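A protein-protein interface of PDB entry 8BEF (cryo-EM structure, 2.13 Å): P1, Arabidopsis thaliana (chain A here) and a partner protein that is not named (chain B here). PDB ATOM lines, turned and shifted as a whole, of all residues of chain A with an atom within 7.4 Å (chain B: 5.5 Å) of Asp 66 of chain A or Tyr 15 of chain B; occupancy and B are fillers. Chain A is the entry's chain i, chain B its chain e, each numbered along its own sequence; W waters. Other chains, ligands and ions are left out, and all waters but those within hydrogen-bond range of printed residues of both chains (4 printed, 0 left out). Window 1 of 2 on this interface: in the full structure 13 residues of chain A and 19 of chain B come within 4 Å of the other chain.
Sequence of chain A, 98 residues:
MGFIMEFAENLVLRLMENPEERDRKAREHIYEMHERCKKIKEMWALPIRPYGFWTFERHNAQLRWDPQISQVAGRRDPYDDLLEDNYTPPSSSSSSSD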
ATOM      1  N   ALA A  61      24.066  19.953 -33.283  1.00  0.00           N
ATOM      2  CA  ALA A  61      23.787  21.368 -33.506  1.00  0.00           C
ATOM      3  C   ALA A  61      23.429  22.082 -32.207  1.00  0.00           C
ATOM      4  O   ALA A  61      23.897  23.198 -31.960  1.00  0.00           O
ATOM      5  CB  ALA A  61      22.667  21.526 -34.535  1.00  0.00           C
ATOM      6  N   GLN A  62      22.607  21.456 -31.359  1.00  0.00           N
ATOM      7  CA  GLN A  62      22.164  22.129 -30.142  1.00  0.00           C
ATOM      8  C   GLN A  62      23.322  22.347 -29.171  1.00  0.00           C
ATOM      9  O   GLN A  62      23.378  23.373 -28.486  1.00  0.00           O
ATOM     10  CB  GLN A  62      21.028  21.342 -29.479  1.00  0.00           C
ATOM     11  CG  GLN A  62      20.701  21.786 -28.055  1.00  0.00           C
ATOM     12  CD  GLN A  62      19.468  21.104 -27.474  1.00  0.00           C
ATOM     13  OE1 GLN A  62      19.215  19.928 -27.723  1.00  0.00           O
ATOM     14  NE2 GLN A  62      18.702  21.847 -26.686  1.00  0.00           N
ATOM     15  N   LEU A  63      24.262  21.400 -29.109  1.00  0.00           N
ATOM     16  CA  LEU A  63      25.423  21.551 -28.236  1.00  0.00           C
ATOM     17  C   LEU A  63      26.258  22.778 -28.577  1.00  0.00           C
ATOM     18  O   LEU A  63      26.972  23.286 -27.709  1.00  0.00           O
ATOM     19  CB  LEU A  63      26.301  20.302 -28.300  1.00  0.00           C
ATOM     20  CG  LEU A  63      25.827  19.055 -27.547  1.00  0.00           C
ATOM     21  CD1 LEU A  63      26.999  18.146 -27.263  1.00  0.00           C
ATOM     22  CD2 LEU A  63      25.118  19.423 -26.259  1.00  0.00           C
ATOM     23  N   ARG A  64      26.193  23.265 -29.817  1.00  0.00           N
ATOM     24  CA  ARG A  64      26.958  24.440 -30.215  1.00  0.00           C
ATOM     25  C   ARG A  64      26.122  25.709 -30.296  1.00  0.00           C
ATOM     26  O   ARG A  64      26.679  26.803 -30.166  1.00  0.00           O
ATOM     27  CB  ARG A  64      27.632  24.200 -31.568  1.00  0.00           C
ATOM     28  CG  ARG A  64      28.205  22.808 -31.725  1.00  0.00           C
ATOM     29  CD  ARG A  64      29.435  22.821 -32.612  1.00  0.00           C
ATOM     30  NE  ARG A  64      29.118  23.172 -33.992  1.00  0.00           N
ATOM     31  CZ  ARG A  64      28.445  22.397 -34.831  1.00  0.00           C
ATOM     32  NH1 ARG A  64      27.989  21.211 -34.464  1.00  0.00           N
ATOM     33  NH2 ARG A  64      28.227  22.821 -36.072  1.00  0.00           N
ATOM     34  N   TRP A  65      24.812  25.589 -30.507  1.00  0.00           N
ATOM     35  CA  TRP A  65      23.955  26.767 -30.591  1.00  0.00           C
ATOM     36  C   TRP A  65      23.544  27.252 -29.207  1.00  0.00           C
ATOM     37  O   TRP A  65      23.687  28.434 -28.891  1.00  0.00           O
ATOM     38  CB  TRP A  65      22.719  26.455 -31.435  1.00  0.00           C
ATOM     39  CG  TRP A  65      21.708  27.557 -31.455  1.00  0.00           C
ATOM     40  CD1 TRP A  65      20.449  27.522 -30.934  1.00  0.00           C
ATOM     41  CD2 TRP A  65      21.863  28.853 -32.042  1.00  0.00           C
ATOM     42  NE1 TRP A  65      19.813  28.719 -31.149  1.00  0.00           N
ATOM     43  CE2 TRP A  65      20.658  29.554 -31.829  1.00  0.00           C
ATOM     44  CE3 TRP A  65      22.905  29.494 -32.717  1.00  0.00           C
ATOM     45  CZ2 TRP A  65      20.468  30.861 -32.268  1.00  0.00           C
ATOM     46  CZ3 TRP A  65      22.712  30.792 -33.155  1.00  0.00           C
ATOM     47  CH2 TRP A  65      21.505  31.461 -32.929  1.00  0.00           C
ATOM     48  N   ASP A  66      23.045  26.343 -28.372  1.00  0.00           N
ATOM     49  CA  ASP A  66      22.516  26.721 -27.064  1.00  0.00           C
ATOM     50  C   ASP A  66      23.490  27.511 -26.193  1.00  0.00           C
ATOM     51  O   ASP A  66      23.031  28.433 -25.498  1.00  0.00           O
ATOM     52  CB  ASP A  66      22.021  25.464 -26.331  1.00  0.00           C
ATOM     53  CG  ASP A  66      20.583  25.111 -26.686  1.00  0.00           C
ATOM     54  OD1 ASP A  66      20.039  25.710 -27.635  1.00  0.00           O
ATOM     55  OD2 ASP A  66      19.994  24.239 -26.016  1.00  0.00           O
ATOM     56  N   PRO A  67      24.798  27.218 -26.153  1.00  0.00           N
ATOM     57  CA  PRO A  67      25.697  28.100 -25.388  1.00  0.00           C
ATOM     58  C   PRO A  67      25.677  29.542 -25.866  1.00  0.00           C
ATOM     59  O   PRO A  67      25.914  30.450 -25.062  1.00  0.00           O
ATOM     60  CB  PRO A  67      27.083  27.465 -25.578  1.00  0.00           C
ATOM     61  CG  PRO A  67      26.833  26.062 -25.973  1.00  0.00           C
ATOM     62  CD  PRO A  67      25.468  25.978 -26.585  1.00  0.00           C
ATOM     63  N   GLN A  68      25.395  29.782 -27.150  1.00  0.00           N
ATOM     64  CA  GLN A  68      25.369  31.147 -27.665  1.00  0.00           C
ATOM     65  C   GLN A  68      24.155  31.935 -27.178  1.00  0.00           C
ATOM     66  O   GLN A  68      24.194  33.169 -27.188  1.00  0.00           O
ATOM     67  CB  GLN A  68      25.405  31.136 -29.198  1.00  0.00           C
ATOM     68  CG  GLN A  68      26.726  30.666 -29.800  1.00  0.00           C
ATOM     69  CD  GLN A  68      26.663  30.529 -31.314  1.00  0.00           C
ATOM     70  OE1 GLN A  68      26.411  31.499 -32.025  1.00  0.00           O
ATOM     71  NE2 GLN A  68      26.881  29.317 -31.811  1.00  0.00           N
ATOM     72  N   ILE A  69      23.083  31.260 -26.766  1.00  0.00           N
ATOM     73  CA  ILE A  69      21.889  31.914 -26.238  1.00  0.00           C
ATOM     74  C   ILE A  69      21.730  31.681 -24.742  1.00  0.00           C
ATOM     75  O   ILE A  69      20.648  31.913 -24.197  1.00  0.00           O
ATOM     76  CB  ILE A  69      20.620  31.469 -26.987  1.00  0.00           C
ATOM     77  CG1 ILE A  69      20.530  29.940 -27.031  1.00  0.00           C
ATOM     78  CG2 ILE A  69      20.561  32.101 -28.375  1.00  0.00           C
ATOM     79  CD1 ILE A  69      19.152  29.410 -27.369  1.00  0.00           C
ATOM     80  N   SER A  70      22.785  31.230 -24.061  1.00  0.00           N
ATOM     81  CA  SER A  70      22.668  30.846 -22.659  1.00  0.00           C
ATOM     82  C   SER A  70      22.406  32.032 -21.738  1.00  0.00           C
ATOM     83  O   SER A  70      21.965  31.829 -20.604  1.00  0.00           O
ATOM     84  CB  SER A  70      23.932  30.103 -22.215  1.00  0.00           C
ATOM     85  OG  SER A  70      25.043  30.976 -22.161  1.00  0.00           O
ATOM     86  N   GLN A  71      22.665  33.254 -22.192  1.00  0.00           N
ATOM     87  CA  GLN A  71      22.428  34.454 -21.403  1.00  0.00           C
ATOM     88  C   GLN A  71      21.142  35.170 -21.799  1.00  0.00           C
ATOM     89  O   GLN A  71      20.920  36.305 -21.372  1.00  0.00           O
ATOM     90  CB  GLN A  71      23.619  35.408 -21.528  1.00  0.00           C
ATOM     91  CG  GLN A  71      24.718  35.184 -20.500  1.00  0.00           C
ATOM     92  CD  GLN A  71      24.816  33.741 -20.049  1.00  0.00           C
ATOM     93  OE1 GLN A  71      25.248  32.870 -20.800  1.00  0.00           O
ATOM     94  NE2 GLN A  71      24.404  33.481 -18.816  1.00  0.00           N
ATOM     95  N   VAL A  72      20.296  34.534 -22.603  1.00  0.00           N
ATOM     96  CA  VAL A  72      19.090  35.173 -23.115  1.00  0.00           C
ATOM     97  C   VAL A  72      17.982  35.075 -22.075  1.00  0.00           C
ATOM     98  O   VAL A  72      17.744  34.005 -21.501  1.00  0.00           O
ATOM     99  CB  VAL A  72      18.665  34.532 -24.447  1.00  0.00           C
ATOM    100  CG1 VAL A  72      17.254  34.954 -24.823  1.00  0.00           C
ATOM    101  CG2 VAL A  72      19.655  34.891 -25.545  1.00  0.00           C
ATOM    102  N   ARG A  75      15.691  31.799 -20.445  1.00  0.00           N
ATOM    103  CA  ARG A  75      16.317  30.497 -20.247  1.00  0.00           C
ATOM    104  C   ARG A  75      17.518  30.564 -19.306  1.00  0.00           C
ATOM    105  O   ARG A  75      18.324  29.628 -19.279  1.00  0.00           O
ATOM    106  CB  ARG A  75      16.738  29.885 -21.592  1.00  0.00           C
ATOM    107  CG  ARG A  75      17.766  30.696 -22.360  1.00  0.00           C
ATOM    108  CD  ARG A  75      17.882  30.219 -23.798  1.00  0.00           C
ATOM    109  NE  ARG A  75      18.524  28.915 -23.901  1.00  0.00           N
ATOM    110  CZ  ARG A  75      17.893  27.789 -24.200  1.00  0.00           C
ATOM    111  NH1 ARG A  75      16.589  27.767 -24.428  1.00  0.00           N
ATOM    112  NH2 ARG A  75      18.585  26.657 -24.272  1.00  0.00           N
ATOM    113  N   ALA B   2      13.821  19.309 -23.195  1.00  0.00           N
ATOM    114  CA  ALA B   2      15.090  19.535 -23.911  1.00  0.00           C
ATOM    115  C   ALA B   2      15.388  20.950 -24.406  1.00  0.00           C
ATOM    116  O   ALA B   2      16.485  21.177 -24.670  1.00  0.00           O
ATOM    117  CB  ALA B   2      15.153  18.511 -25.016  1.00  0.00           C
ATOM    118  N   SER B   3      14.353  21.756 -24.660  1.00  0.00           N
ATOM    119  CA  SER B   3      14.544  23.090 -25.287  1.00  0.00           C
ATOM    120  C   SER B   3      15.283  24.052 -24.361  1.00  0.00           C
ATOM    121  O   SER B   3      15.915  24.941 -24.873  1.00  0.00           O
ATOM    122  CB  SER B   3      13.176  23.690 -25.740  1.00  0.00           C
ATOM    123  OG  SER B   3      12.494  24.306 -24.665  1.00  0.00           O
ATOM    124  N   GLY B   4      15.056  23.941 -23.057  1.00  0.00           N
ATOM    125  CA  GLY B   4      15.604  24.920 -22.108  1.00  0.00           C
ATOM    126  C   GLY B   4      14.737  26.121 -21.763  1.00  0.00           C
ATOM    127  O   GLY B   4      15.038  26.773 -20.799  1.00  0.00           O
ATOM    128  N   LYS B  11      15.502  28.986 -16.966  1.00  0.00           N
ATOM    129  CA  LYS B  11      15.927  27.700 -17.501  1.00  0.00           C
ATOM    130  C   LYS B  11      14.978  26.599 -17.043  1.00  0.00           C
ATOM    131  O   LYS B  11      14.568  26.555 -15.882  1.00  0.00           O
ATOM    132  CB  LYS B  11      17.359  27.380 -17.059  1.00  0.00           C
ATOM    133  CG  LYS B  11      17.816  25.970 -17.410  1.00  0.00           C
ATOM    134  CD  LYS B  11      19.042  25.544 -16.605  1.00  0.00           C
ATOM    135  CE  LYS B  11      20.215  26.476 -16.845  1.00  0.00           C
ATOM    136  NZ  LYS B  11      20.358  26.823 -18.280  1.00  0.00           N
ATOM    137  N   GLY B  12      14.569  25.802 -18.011  1.00  0.00           N
ATOM    138  CA  GLY B  12      13.711  24.643 -17.716  1.00  0.00           C
ATOM    139  C   GLY B  12      14.253  23.745 -16.601  1.00  0.00           C
ATOM    140  O   GLY B  12      15.465  23.622 -16.560  1.00  0.00           O
ATOM    141  N   ARG B  13      13.396  23.035 -15.866  1.00  0.00           N
ATOM    142  CA  ARG B  13      13.777  22.231 -14.706  1.00  0.00           C
ATOM    143  C   ARG B  13      14.766  21.131 -15.077  1.00  0.00           C
ATOM    144  O   ARG B  13      15.726  20.877 -14.341  1.00  0.00           O
ATOM    145  CB  ARG B  13      12.528  21.629 -14.054  1.00  0.00           C
ATOM    146  CG  ARG B  13      12.804  20.373 -13.226  1.00  0.00           C
ATOM    147  CD  ARG B  13      11.557  19.840 -12.534  1.00  0.00           C
ATOM    148  NE  ARG B  13      10.953  18.724 -13.251  1.00  0.00           N
ATOM    149  CZ  ARG B  13       9.802  18.800 -13.906  1.00  0.00           C
ATOM    150  NH1 ARG B  13       9.104  19.923 -13.943  1.00  0.00           N
ATOM    151  NH2 ARG B  13       9.339  17.724 -14.534  1.00  0.00           N
ATOM    152  N   CYS B  14      14.516  20.432 -16.191  1.00  0.00           N
ATOM    153  CA  CYS B  14      15.268  19.247 -16.656  1.00  0.00           C
ATOM    154  C   CYS B  14      16.327  19.524 -17.754  1.00  0.00           C
ATOM    155  O   CYS B  14      16.895  18.612 -18.211  1.00  0.00           O
ATOM    156  CB  CYS B  14      14.252  18.227 -17.145  1.00  0.00           C
ATOM    157  SG  CYS B  14      13.037  17.791 -15.882  1.00  0.00           S
ATOM    158  N   TYR B  15      16.596  20.758 -18.061  1.00  0.00           N
ATOM    159  CA  TYR B  15      17.538  21.169 -19.122  1.00  0.00           C
ATOM    160  C   TYR B  15      19.021  20.851 -18.803  1.00  0.00           C
ATOM    161  O   TYR B  15      19.644  20.398 -19.695  1.00  0.00           O
ATOM    162  CB  TYR B  15      17.334  22.645 -19.442  1.00  0.00           C
ATOM    163  CG  TYR B  15      18.245  23.108 -20.536  1.00  0.00           C
ATOM    164  CD1 TYR B  15      18.042  22.683 -21.836  1.00  0.00           C
ATOM    165  CD2 TYR B  15      19.334  23.909 -20.257  1.00  0.00           C
ATOM    166  CE1 TYR B  15      18.868  23.103 -22.858  1.00  0.00           C
ATOM    167  CE2 TYR B  15      20.170  24.345 -21.265  1.00  0.00           C
ATOM    168  CZ  TYR B  15      19.925  23.940 -22.564  1.00  0.00           C
ATOM    169  OH  TYR B  15      20.753  24.328 -23.552  1.00  0.00           O
ATOM    170  N   ASP B  16      19.483  20.987 -17.573  1.00  0.00           N
ATOM    171  CA  ASP B  16      20.862  20.618 -17.278  1.00  0.00           C
ATOM    172  C   ASP B  16      21.074  19.114 -17.421  1.00  0.00           C
ATOM    173  O   ASP B  16      22.101  18.676 -17.952  1.00  0.00           O
ATOM    174  CB  ASP B  16      21.236  21.114 -15.885  1.00  0.00           C
ATOM    175  CG  ASP B  16      21.471  22.613 -15.856  1.00  0.00           C
ATOM    176  OD1 ASP B  16      21.718  23.189 -16.934  1.00  0.00           O
ATOM    177  OD2 ASP B  16      21.393  23.220 -14.771  1.00  0.00           O
ATOM    178  N   PHE B  17      20.100  18.310 -16.984  1.00  0.00           N
ATOM    179  CA  PHE B  17      20.174  16.868 -17.205  1.00  0.00           C
ATOM    180  C   PHE B  17      20.209  16.544 -18.692  1.00  0.00           C
ATOM    181  O   PHE B  17      20.997  15.698 -19.138  1.00  0.00           O
ATOM    182  CB  PHE B  17      18.981  16.170 -16.552  1.00  0.00           C
ATOM    183  CG  PHE B  17      19.069  16.071 -15.059  1.00  0.00           C
ATOM    184  CD1 PHE B  17      20.005  15.249 -14.455  1.00  0.00           C
ATOM    185  CD2 PHE B  17      18.194  16.784 -14.256  1.00  0.00           C
ATOM    186  CE1 PHE B  17      20.077  15.157 -13.076  1.00  0.00           C
ATOM    187  CE2 PHE B  17      18.261  16.694 -12.879  1.00  0.00           C
ATOM    188  CZ  PHE B  17      19.202  15.882 -12.289  1.00  0.00           C
ATOM    189  N   TRP B  18      19.330  17.203 -19.450  1.00  0.00           N
ATOM    190  CA  TRP B  18      19.328  17.027 -20.908  1.00  0.00           C
ATOM    191  C   TRP B  18      20.722  17.326 -21.496  1.00  0.00           C
ATOM    192  O   TRP B  18      21.123  16.600 -22.339  1.00  0.00           O
ATOM    193  CB  TRP B  18      18.238  17.872 -21.595  1.00  0.00           C
ATOM    194  CG  TRP B  18      18.404  17.808 -23.078  1.00  0.00           C
ATOM    195  CD1 TRP B  18      18.897  18.768 -23.911  1.00  0.00           C
ATOM    196  CD2 TRP B  18      18.178  16.652 -23.889  1.00  0.00           C
ATOM    197  NE1 TRP B  18      18.960  18.293 -25.188  1.00  0.00           N
ATOM    198  CE2 TRP B  18      18.520  17.001 -25.211  1.00  0.00           C
ATOM    199  CE3 TRP B  18      17.706  15.366 -23.625  1.00  0.00           C
ATOM    200  CZ2 TRP B  18      18.408  16.099 -26.261  1.00  0.00           C
ATOM    201  CZ3 TRP B  18      17.596  14.483 -24.666  1.00  0.00           C
ATOM    202  CH2 TRP B  18      17.934  14.844 -25.969  1.00  0.00           C
ATOM    203  N   MET B  19      21.304  18.425 -21.106  1.00  0.00           N
ATOM    204  CA  MET B  19      22.565  18.844 -21.705  1.00  0.00           C
ATOM    205  C   MET B  19      23.700  17.910 -21.309  1.00  0.00           C
ATOM    206  O   MET B  19      24.577  17.620 -22.129  1.00  0.00           O
ATOM    207  CB  MET B  19      22.877  20.289 -21.317  1.00  0.00           C
ATOM    208  CG  MET B  19      21.945  21.299 -21.962  1.00  0.00           C
ATOM    209  SD  MET B  19      21.774  21.108 -23.751  1.00  0.00           S
ATOM    210  CE  MET B  19      23.330  21.787 -24.301  1.00  0.00           C
ATOM    211  N   ASP B  20      23.700  17.413 -20.067  1.00  0.00           N
ATOM    212  CA  ASP B  20      24.682  16.397 -19.691  1.00  0.00           C
ATOM    213  C   ASP B  20      24.529  15.148 -20.548  1.00  0.00           C
ATOM    214  O   ASP B  20      25.517  14.600 -21.051  1.00  0.00           O
ATOM    215  CB  ASP B  20      24.561  16.036 -18.207  1.00  0.00           C
ATOM    216  CG  ASP B  20      24.551  17.244 -17.307  1.00  0.00           C
ATOM    217  OD1 ASP B  20      25.304  18.198 -17.585  1.00  0.00           O
ATOM    218  OD2 ASP B  20      23.799  17.237 -16.308  1.00  0.00           O
HETATM  219  O   HOH W   1      20.985  29.570 -19.517  1.00  0.00           O
HETATM  220  O   HOH W   2      20.886  17.840 -27.717  1.00  0.00           O
HETATM  221  O   HOH W   3      18.076  26.781 -20.809  1.00  0.00           O
HETATM  222  O   HOH W   4      16.983  25.222 -27.511  1.00  0.00           O
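The backbone NH (N) of Gly 12 of chain B lies within hydrogen-bond range of the backbone carbonyl oxygen (O) of Gly 4 of chain B (3.0 Å). The side-chain sulfur of Met 19 of chain B is in hydrogen-bond range of the side-chain hydroxyl of Tyr 15 of chain B (3.4 Å). NE2 of Gln 62 of chain A is in hydrogen-bond range of OD2 of Asp 66 of chain A (2.8 Å). The side-chain carboxylate of Asp 66 of chain A is in salt-bridge range of the guanidinium group of Arg 75 of chain A (3.3 Å).
The backbone carbonyl oxygen of Ala 2 of chain B sits at hydrogen-bond distance from the side-chain amide nitrogen of Gln 62 of chain A (3.1 Å). The guanidinium group (NH1) of Arg 75 of chain A lies within hydrogen-bond range of the backbone carbonyl oxygen (O) of Ser 3 of chain B. The side-chain hydroxyl (OH) of Tyr 15 of chain B sits at hydrogen-bond distance from the side-chain carboxylate (OD2) of Asp 66 of chain A (2.6 Å). The side-chain hydroxyl (OH) of Tyr 15 of chain B sits at hydrogen-bond distance from the guanidinium group (NH2) of Arg 75 of chain A (3.3 Å). The indole nitrogen (NE1) of Trp 18 of chain B is in hydrogen-bond range of the side-chain amide oxygen (OE1) of Gln 62 of chain A (3.0 Å).
Water W1 lies within hydrogen-bond range of O of Arg 75 of chain A (2.7 Å), O of Ser 70 of chain A (2.7 Å) and NZ of Lys 11 of chain B (3.1 Å). Water W2 lies within hydrogen-bond range of the side-chain amide oxygen of Gln 62 of chain A (2.7 Å) and the indole nitrogen of Trp 18 of chain B (3.2 Å). Water W4 bridges O of Ser 3 of chain B (2.9 Å) and OD1 of Asp 66 of chain A (3.1 Å). Water W3 lies within hydrogen-bond range of O of Gly 4 of chain B (3.0 Å), O of Arg 75 of chain A (3.2 Å) and NZ of Lys 11 of chain B (3.4 Å).
Met 19 of chain B touches Leu 63 of chain A (CE to CD2, 3.6 Å). CB of Arg 75 of chain A touches O of Gly 4 of chain B, 3.6 Å away. CB of Lys 11 of chain B touches O of Arg 75 of chain A (3.3 Å).
Printed residues of chain B within 4 Å of Asp 66 of chain A: Tyr 15. Tyr 15 of chain B touches just these residues of chain A: Asp 66 and Arg 75. Of the printed residues of chain A, Trp 18 of chain B touches Gln 62. Of the printed residues of chain A, Gly 4 of chain B touches Arg 75. Printed residues of chain B within 4 Å of Leu 63 of chain A: Met 19. Of the printed residues of chain A, Lys 11 of chain B touches Arg 75. The nearest residue of chain B that does not touch Asp 66 of chain A is Met 19 of chain B (4.3 Å). The nearest residue of chain A that does not touch Tyr 15 of chain B is Gln 62 of chain A (4.03 Å).
Hydrophobic or aromatic side chains of chain B that line the printed part of chain A: Tyr 15, Trp 18 and Met 19. Of the 13 printed residues of chain A, 4 touch a printed residue of chain B. Printed residues of chain A that touch a printed residue of chain B: Gln 62, Leu 63, Asp 66 and Arg 75. Hydrophobic or aromatic side chains of chain A within 4 Å of the printed part of chain B: Leu 63. Among the printed residues, 8 pairs touch across the chains.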
